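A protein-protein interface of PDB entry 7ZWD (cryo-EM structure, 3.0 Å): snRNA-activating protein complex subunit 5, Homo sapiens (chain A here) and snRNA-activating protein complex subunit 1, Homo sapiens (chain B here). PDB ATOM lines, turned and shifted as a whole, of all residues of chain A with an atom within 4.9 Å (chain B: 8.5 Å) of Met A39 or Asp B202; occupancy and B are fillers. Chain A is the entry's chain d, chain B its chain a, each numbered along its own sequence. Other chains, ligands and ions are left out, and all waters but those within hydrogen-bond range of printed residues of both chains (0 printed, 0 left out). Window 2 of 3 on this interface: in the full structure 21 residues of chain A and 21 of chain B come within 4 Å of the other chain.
The side-chain carboxylate (OD2) of Asp B202 sits close to the side-chain sulfur (SD) of Met A39 (3.8 Å). The side-chain carboxylate of Asp B202 is in salt-bridge range of the guanidinium group of Arg A43 (3.4 Å).
Of the 18 printed residues of chain B, 5 touch a printed residue of chain A. Printed residues of chain B that touch a printed residue of chain A: Ile B194, Val B196, Asp B202, Ala B204 and Leu B205. Among the printed residues, 6 pairs touch across the chains. Among the printed residues, Asp or Glu carboxylates within 4 Å of a Lys or Arg side-chain nitrogen of the other chain: Arg A43 with Asp B202.
CB of Ala A35 touches O of Ala B204, 3.5 Å away. Leu A36 touches Leu B205 (CD2 to CD1, 3.5 Å). Arg A43 touches Ile B194. Arg A43 touches Val B196.
The side-chain hydroxyl of Ser A38 is in hydrogen-bond range of the backbone carbonyl oxygen of Ala A35. O of Met A39 lies within hydrogen-bond range of OG of Ser A42. The side-chain sulfur of Met A39 sits at hydrogen-bond distance from the guanidinium group of Arg A43 (3.1 Å).
Of the printed residues of chain B, Leu A36 touches Leu B205. No residue of chain B comes within 4 Å of Ser A38. Of chain B, only Asp B202 (3.8 Å) comes within 4 Å of Met A39. Val B193 touches none of the printed residues of chain A. Of the printed residues of chain A, Ile B194 touches Arg A43 (3.7 Å). Asp B202 touches just these residues of chain A: Met A39 and Arg A43. The nearest residue of chain B that does not touch Met A39 is Ile B194 (4.8 Å). The nearest printed residue of chain A that does not touch Asp B202 is Leu A36 (6.8 Å).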
ATOM      1  N   ALA A  35      -8.493  -8.166  20.137  1.00  0.00           N
ATOM      2  CA  ALA A  35      -9.547  -7.160  20.253  1.00  0.00           C
ATOM      3  C   ALA A  35      -9.942  -6.938  21.710  1.00  0.00           C
ATOM      4  O   ALA A  35     -10.131  -5.794  22.146  1.00  0.00           O
ATOM      5  CB  ALA A  35     -10.761  -7.574  19.422  1.00  0.00           C
ATOM      6  N   LEU A  36     -10.067  -8.025  22.478  1.00  0.00           N
ATOM      7  CA  LEU A  36     -10.379  -7.911  23.897  1.00  0.00           C
ATOM      8  C   LEU A  36      -9.297  -7.155  24.648  1.00  0.00           C
ATOM      9  O   LEU A  36      -9.612  -6.298  25.476  1.00  0.00           O
ATOM     10  CB  LEU A  36     -10.558  -9.292  24.535  1.00  0.00           C
ATOM     11  CG  LEU A  36     -11.505 -10.344  23.963  1.00  0.00           C
ATOM     12  CD1 LEU A  36     -11.691 -11.483  24.945  1.00  0.00           C
ATOM     13  CD2 LEU A  36     -12.834  -9.721  23.615  1.00  0.00           C
ATOM     14  N   GLN A  37      -8.026  -7.469  24.385  1.00  0.00           N
ATOM     15  CA  GLN A  37      -6.938  -6.762  25.056  1.00  0.00           C
ATOM     16  C   GLN A  37      -6.989  -5.272  24.749  1.00  0.00           C
ATOM     17  O   GLN A  37      -6.866  -4.433  25.653  1.00  0.00           O
ATOM     18  CB  GLN A  37      -5.581  -7.348  24.650  1.00  0.00           C
ATOM     19  CG  GLN A  37      -5.434  -8.867  24.759  1.00  0.00           C
ATOM     20  CD  GLN A  37      -6.229  -9.493  25.896  1.00  0.00           C
ATOM     21  OE1 GLN A  37      -6.206  -9.013  27.030  1.00  0.00           O
ATOM     22  NE2 GLN A  37      -6.943 -10.570  25.590  1.00  0.00           N
ATOM     23  N   SER A  38      -7.190  -4.925  23.475  1.00  0.00           N
ATOM     24  CA  SER A  38      -7.285  -3.521  23.093  1.00  0.00           C
ATOM     25  C   SER A  38      -8.421  -2.824  23.834  1.00  0.00           C
ATOM     26  O   SER A  38      -8.234  -1.745  24.416  1.00  0.00           O
ATOM     27  CB  SER A  38      -7.474  -3.401  21.581  1.00  0.00           C
ATOM     28  OG  SER A  38      -8.805  -3.711  21.206  1.00  0.00           O
ATOM     29  N   MET A  39      -9.608  -3.441  23.851  1.00  0.00           N
ATOM     30  CA  MET A  39     -10.750  -2.736  24.423  1.00  0.00           C
ATOM     31  C   MET A  39     -10.662  -2.675  25.943  1.00  0.00           C
ATOM     32  O   MET A  39     -11.117  -1.701  26.550  1.00  0.00           O
ATOM     33  CB  MET A  39     -12.071  -3.375  23.991  1.00  0.00           C
ATOM     34  CG  MET A  39     -12.296  -4.804  24.430  1.00  0.00           C
ATOM     35  SD  MET A  39     -14.073  -5.094  24.550  1.00  0.00           S
ATOM     36  CE  MET A  39     -14.121  -6.803  25.061  1.00  0.00           C
ATOM     37  N   ILE A  40     -10.067  -3.685  26.585  1.00  0.00           N
ATOM     38  CA  ILE A  40      -9.954  -3.614  28.039  1.00  0.00           C
ATOM     39  C   ILE A  40      -8.900  -2.591  28.431  1.00  0.00           C
ATOM     40  O   ILE A  40      -9.046  -1.899  29.441  1.00  0.00           O
ATOM     41  CB  ILE A  40      -9.657  -4.989  28.666  1.00  0.00           C
ATOM     42  CG1 ILE A  40      -8.366  -5.585  28.112  1.00  0.00           C
ATOM     43  CG2 ILE A  40     -10.823  -5.932  28.443  1.00  0.00           C
ATOM     44  CD1 ILE A  40      -8.063  -6.959  28.637  1.00  0.00           C
ATOM     45  N   SER A  41      -7.827  -2.466  27.645  1.00  0.00           N
ATOM     46  CA  SER A  41      -6.889  -1.376  27.889  1.00  0.00           C
ATOM     47  C   SER A  41      -7.595  -0.031  27.767  1.00  0.00           C
ATOM     48  O   SER A  41      -7.435   0.851  28.620  1.00  0.00           O
ATOM     49  CB  SER A  41      -5.711  -1.464  26.918  1.00  0.00           C
ATOM     50  OG  SER A  41      -6.157  -1.714  25.596  1.00  0.00           O
ATOM     51  N   SER A  42      -8.421   0.121  26.728  1.00  0.00           N
ATOM     52  CA  SER A  42      -9.138   1.379  26.535  1.00  0.00           C
ATOM     53  C   SER A  42     -10.109   1.658  27.678  1.00  0.00           C
ATOM     54  O   SER A  42     -10.284   2.814  28.081  1.00  0.00           O
ATOM     55  CB  SER A  42      -9.880   1.358  25.199  1.00  0.00           C
ATOM     56  OG  SER A  42     -11.029   0.532  25.268  1.00  0.00           O
ATOM     57  N   ARG A  43     -10.753   0.617  28.215  1.00  0.00           N
ATOM     58  CA  ARG A  43     -11.765   0.822  29.244  1.00  0.00           C
ATOM     59  C   ARG A  43     -11.185   0.975  30.646  1.00  0.00           C
ATOM     60  O   ARG A  43     -11.739   1.742  31.440  1.00  0.00           O
ATOM     61  CB  ARG A  43     -12.793  -0.313  29.221  1.00  0.00           C
ATOM     62  CG  ARG A  43     -13.718  -0.260  28.012  1.00  0.00           C
ATOM     63  CD  ARG A  43     -14.121  -1.639  27.523  1.00  0.00           C
ATOM     64  NE  ARG A  43     -15.230  -2.181  28.301  1.00  0.00           N
ATOM     65  CZ  ARG A  43     -16.050  -3.135  27.872  1.00  0.00           C
ATOM     66  NH1 ARG A  43     -15.892  -3.653  26.661  1.00  0.00           N
ATOM     67  NH2 ARG A  43     -17.033  -3.566  28.651  1.00  0.00           N
ATOM     68  N   MET B 190     -22.605 -15.061  27.294  1.00  0.00           N
ATOM     69  CA  MET B 190     -21.741 -14.123  28.005  1.00  0.00           C
ATOM     70  C   MET B 190     -21.396 -12.911  27.143  1.00  0.00           C
ATOM     71  O   MET B 190     -21.182 -11.818  27.677  1.00  0.00           O
ATOM     72  CB  MET B 190     -20.477 -14.820  28.512  1.00  0.00           C
ATOM     73  CG  MET B 190     -19.730 -15.619  27.484  1.00  0.00           C
ATOM     74  SD  MET B 190     -18.422 -14.683  26.686  1.00  0.00           S
ATOM     75  CE  MET B 190     -17.149 -14.806  27.931  1.00  0.00           C
ATOM     76  N   LYS B 191     -21.338 -13.073  25.814  1.00  0.00           N
ATOM     77  CA  LYS B 191     -21.328 -11.896  24.947  1.00  0.00           C
ATOM     78  C   LYS B 191     -22.491 -10.966  25.239  1.00  0.00           C
ATOM     79  O   LYS B 191     -22.306  -9.744  25.262  1.00  0.00           O
ATOM     80  CB  LYS B 191     -21.400 -12.277  23.466  1.00  0.00           C
ATOM     81  CG  LYS B 191     -20.334 -13.205  22.948  1.00  0.00           C
ATOM     82  CD  LYS B 191     -19.304 -12.439  22.148  1.00  0.00           C
ATOM     83  CE  LYS B 191     -18.309 -13.379  21.506  1.00  0.00           C
ATOM     84  NZ  LYS B 191     -18.961 -14.291  20.531  1.00  0.00           N
ATOM     85  N   HIS B 192     -23.685 -11.521  25.451  1.00  0.00           N
ATOM     86  CA  HIS B 192     -24.857 -10.675  25.654  1.00  0.00           C
ATOM     87  C   HIS B 192     -24.784  -9.874  26.951  1.00  0.00           C
ATOM     88  O   HIS B 192     -25.552  -8.920  27.122  1.00  0.00           O
ATOM     89  CB  HIS B 192     -26.136 -11.513  25.616  1.00  0.00           C
ATOM     90  CG  HIS B 192     -26.300 -12.314  24.362  1.00  0.00           C
ATOM     91  ND1 HIS B 192     -26.366 -13.690  24.357  1.00  0.00           N
ATOM     92  CD2 HIS B 192     -26.416 -11.928  23.069  1.00  0.00           C
ATOM     93  CE1 HIS B 192     -26.515 -14.118  23.117  1.00  0.00           C
ATOM     94  NE2 HIS B 192     -26.548 -13.069  22.316  1.00  0.00           N
ATOM     95  N   VAL B 193     -23.884 -10.221  27.867  1.00  0.00           N
ATOM     96  CA  VAL B 193     -23.801  -9.540  29.154  1.00  0.00           C
ATOM     97  C   VAL B 193     -22.515  -8.733  29.295  1.00  0.00           C
ATOM     98  O   VAL B 193     -22.446  -7.824  30.123  1.00  0.00           O
ATOM     99  CB  VAL B 193     -23.959 -10.543  30.318  1.00  0.00           C
ATOM    100  CG1 VAL B 193     -25.308 -11.244  30.240  1.00  0.00           C
ATOM    101  CG2 VAL B 193     -22.821 -11.546  30.333  1.00  0.00           C
ATOM    102  N   ILE B 194     -21.478  -9.040  28.508  1.00  0.00           N
ATOM    103  CA  ILE B 194     -20.232  -8.284  28.633  1.00  0.00           C
ATOM    104  C   ILE B 194     -20.402  -6.850  28.143  1.00  0.00           C
ATOM    105  O   ILE B 194     -19.837  -5.916  28.727  1.00  0.00           O
ATOM    106  CB  ILE B 194     -19.076  -8.995  27.899  1.00  0.00           C
ATOM    107  CG1 ILE B 194     -18.667 -10.264  28.647  1.00  0.00           C
ATOM    108  CG2 ILE B 194     -17.879  -8.071  27.727  1.00  0.00           C
ATOM    109  CD1 ILE B 194     -18.151 -11.348  27.748  1.00  0.00           C
ATOM    110  N   SER B 195     -21.181  -6.646  27.082  1.00  0.00           N
ATOM    111  CA  SER B 195     -21.341  -5.312  26.522  1.00  0.00           C
ATOM    112  C   SER B 195     -21.921  -4.354  27.557  1.00  0.00           C
ATOM    113  O   SER B 195     -22.721  -4.738  28.415  1.00  0.00           O
ATOM    114  CB  SER B 195     -22.240  -5.357  25.286  1.00  0.00           C
ATOM    115  OG  SER B 195     -23.362  -6.194  25.502  1.00  0.00           O
ATOM    116  N   VAL B 196     -21.499  -3.090  27.472  1.00  0.00           N
ATOM    117  CA  VAL B 196     -21.954  -2.088  28.430  1.00  0.00           C
ATOM    118  C   VAL B 196     -23.436  -1.792  28.245  1.00  0.00           C
ATOM    119  O   VAL B 196     -24.092  -1.274  29.157  1.00  0.00           O
ATOM    120  CB  VAL B 196     -21.106  -0.808  28.312  1.00  0.00           C
ATOM    121  CG1 VAL B 196     -19.719  -1.033  28.896  1.00  0.00           C
ATOM    122  CG2 VAL B 196     -21.014  -0.365  26.858  1.00  0.00           C
ATOM    123  N   ASP B 197     -23.987  -2.108  27.076  1.00  0.00           N
ATOM    124  CA  ASP B 197     -25.399  -1.911  26.786  1.00  0.00           C
ATOM    125  C   ASP B 197     -26.028  -3.253  26.440  1.00  0.00           C
ATOM    126  O   ASP B 197     -25.379  -4.110  25.832  1.00  0.00           O
ATOM    127  CB  ASP B 197     -25.595  -0.915  25.640  1.00  0.00           C
ATOM    128  CG  ASP B 197     -24.997  -1.401  24.337  1.00  0.00           C
ATOM    129  OD1 ASP B 197     -23.753  -1.420  24.222  1.00  0.00           O
ATOM    130  OD2 ASP B 197     -25.771  -1.763  23.428  1.00  0.00           O
ATOM    131  N   LYS B 198     -27.290  -3.431  26.835  1.00  0.00           N
ATOM    132  CA  LYS B 198     -27.994  -4.687  26.605  1.00  0.00           C
ATOM    133  C   LYS B 198     -28.522  -4.815  25.183  1.00  0.00           C
ATOM    134  O   LYS B 198     -28.769  -5.936  24.725  1.00  0.00           O
ATOM    135  CB  LYS B 198     -29.151  -4.819  27.598  1.00  0.00           C
ATOM    136  CG  LYS B 198     -29.729  -6.219  27.731  1.00  0.00           C
ATOM    137  CD  LYS B 198     -28.654  -7.241  28.066  1.00  0.00           C
ATOM    138  CE  LYS B 198     -29.006  -8.610  27.511  1.00  0.00           C
ATOM    139  NZ  LYS B 198     -27.902  -9.590  27.699  1.00  0.00           N
ATOM    140  N   SER B 199     -28.699  -3.696  24.476  1.00  0.00           N
ATOM    141  CA  SER B 199     -29.314  -3.740  23.152  1.00  0.00           C
ATOM    142  C   SER B 199     -28.403  -4.419  22.135  1.00  0.00           C
ATOM    143  O   SER B 199     -28.842  -5.290  21.376  1.00  0.00           O
ATOM    144  CB  SER B 199     -29.669  -2.324  22.696  1.00  0.00           C
ATOM    145  OG  SER B 199     -28.568  -1.707  22.051  1.00  0.00           O
ATOM    146  N   LYS B 200     -27.130  -4.032  22.105  1.00  0.00           N
ATOM    147  CA  LYS B 200     -26.219  -4.543  21.088  1.00  0.00           C
ATOM    148  C   LYS B 200     -24.832  -4.804  21.666  1.00  0.00           C
ATOM    149  O   LYS B 200     -24.351  -4.039  22.512  1.00  0.00           O
ATOM    150  CB  LYS B 200     -26.157  -3.568  19.904  1.00  0.00           C
ATOM    151  CG  LYS B 200     -25.728  -2.135  20.241  1.00  0.00           C
ATOM    152  CD  LYS B 200     -24.219  -1.931  20.190  1.00  0.00           C
ATOM    153  CE  LYS B 200     -23.835  -0.511  20.581  1.00  0.00           C
ATOM    154  NZ  LYS B 200     -22.361  -0.341  20.713  1.00  0.00           N
ATOM    155  N   PRO B 201     -24.170  -5.890  21.252  1.00  0.00           N
ATOM    156  CA  PRO B 201     -22.802  -6.148  21.723  1.00  0.00           C
ATOM    157  C   PRO B 201     -21.796  -5.183  21.118  1.00  0.00           C
ATOM    158  O   PRO B 201     -22.146  -4.371  20.256  1.00  0.00           O
ATOM    159  CB  PRO B 201     -22.536  -7.591  21.267  1.00  0.00           C
ATOM    160  CG  PRO B 201     -23.890  -8.162  20.951  1.00  0.00           C
ATOM    161  CD  PRO B 201     -24.695  -7.006  20.453  1.00  0.00           C
ATOM    162  N   ASP B 202     -20.542  -5.266  21.556  1.00  0.00           N
ATOM    163  CA  ASP B 202     -19.515  -4.368  21.053  1.00  0.00           C
ATOM    164  C   ASP B 202     -19.190  -4.686  19.595  1.00  0.00           C
ATOM    165  O   ASP B 202     -19.416  -5.795  19.103  1.00  0.00           O
ATOM    166  CB  ASP B 202     -18.254  -4.467  21.909  1.00  0.00           C
ATOM    167  CG  ASP B 202     -18.553  -4.420  23.394  1.00  0.00           C
ATOM    168  OD1 ASP B 202     -19.536  -3.755  23.781  1.00  0.00           O
ATOM    169  OD2 ASP B 202     -17.806  -5.049  24.173  1.00  0.00           O
ATOM    170  N   LYS B 203     -18.649  -3.686  18.901  1.00  0.00           N
ATOM    171  CA  LYS B 203     -18.280  -3.817  17.499  1.00  0.00           C
ATOM    172  C   LYS B 203     -16.901  -4.429  17.301  1.00  0.00           C
ATOM    173  O   LYS B 203     -16.474  -4.602  16.155  1.00  0.00           O
ATOM    174  CB  LYS B 203     -18.342  -2.452  16.804  1.00  0.00           C
ATOM    175  CG  LYS B 203     -19.716  -1.796  16.821  1.00  0.00           C
ATOM    176  CD  LYS B 203     -20.825  -2.808  16.572  1.00  0.00           C
ATOM    177  CE  LYS B 203     -22.123  -2.375  17.233  1.00  0.00           C
ATOM    178  NZ  LYS B 203     -23.038  -3.523  17.475  1.00  0.00           N
ATOM    179  N   ALA B 204     -16.196  -4.759  18.383  1.00  0.00           N
ATOM    180  CA  ALA B 204     -14.910  -5.433  18.291  1.00  0.00           C
ATOM    181  C   ALA B 204     -15.014  -6.941  18.450  1.00  0.00           C
ATOM    182  O   ALA B 204     -14.037  -7.644  18.169  1.00  0.00           O
ATOM    183  CB  ALA B 204     -13.940  -4.879  19.344  1.00  0.00           C
ATOM    184  N   LEU B 205     -16.162  -7.457  18.886  1.00  0.00           N
ATOM    185  CA  LEU B 205     -16.354  -8.887  19.098  1.00  0.00           C
ATOM    186  C   LEU B 205     -17.589  -9.340  18.330  1.00  0.00           C
ATOM    187  O   LEU B 205     -18.679  -9.438  18.902  1.00  0.00           O
ATOM    188  CB  LEU B 205     -16.489  -9.200  20.587  1.00  0.00           C
ATOM    189  CG  LEU B 205     -15.976 -10.567  21.029  1.00  0.00           C
ATOM    190  CD1 LEU B 205     -14.520 -10.707  20.653  1.00  0.00           C
ATOM    191  CD2 LEU B 205     -16.151 -10.718  22.527  1.00  0.00           C
ATOM    192  N   SER B 206     -17.415  -9.618  17.038  1.00  0.00           N
ATOM    193  CA  SER B 206     -18.486 -10.156  16.211  1.00  0.00           C
ATOM    194  C   SER B 206     -17.927 -11.183  15.236  1.00  0.00           C
ATOM    195  O   SER B 206     -18.580 -11.537  14.250  1.00  0.00           O
ATOM    196  CB  SER B 206     -19.200  -9.034  15.454  1.00  0.00           C
ATOM    197  OG  SER B 206     -19.465  -7.933  16.304  1.00  0.00           O
ATOM    198  N   LEU B 207     -16.715 -11.664  15.508  1.00  0.00           N
ATOM    199  CA  LEU B 207     -15.977 -12.518  14.588  1.00  0.00           C
ATOM    200  C   LEU B 207     -16.203 -14.003  14.871  1.00  0.00           C
ATOM    201  O   LEU B 207     -15.645 -14.858  14.174  1.00  0.00           O
ATOM    202  CB  LEU B 207     -14.489 -12.151  14.648  1.00  0.00           C
ATOM    203  CG  LEU B 207     -13.356 -13.005  14.071  1.00  0.00           C
ATOM    204  CD1 LEU B 207     -13.347 -12.937  12.552  1.00  0.00           C
ATOM    205  CD2 LEU B 207     -12.029 -12.550  14.633  1.00  0.00           C
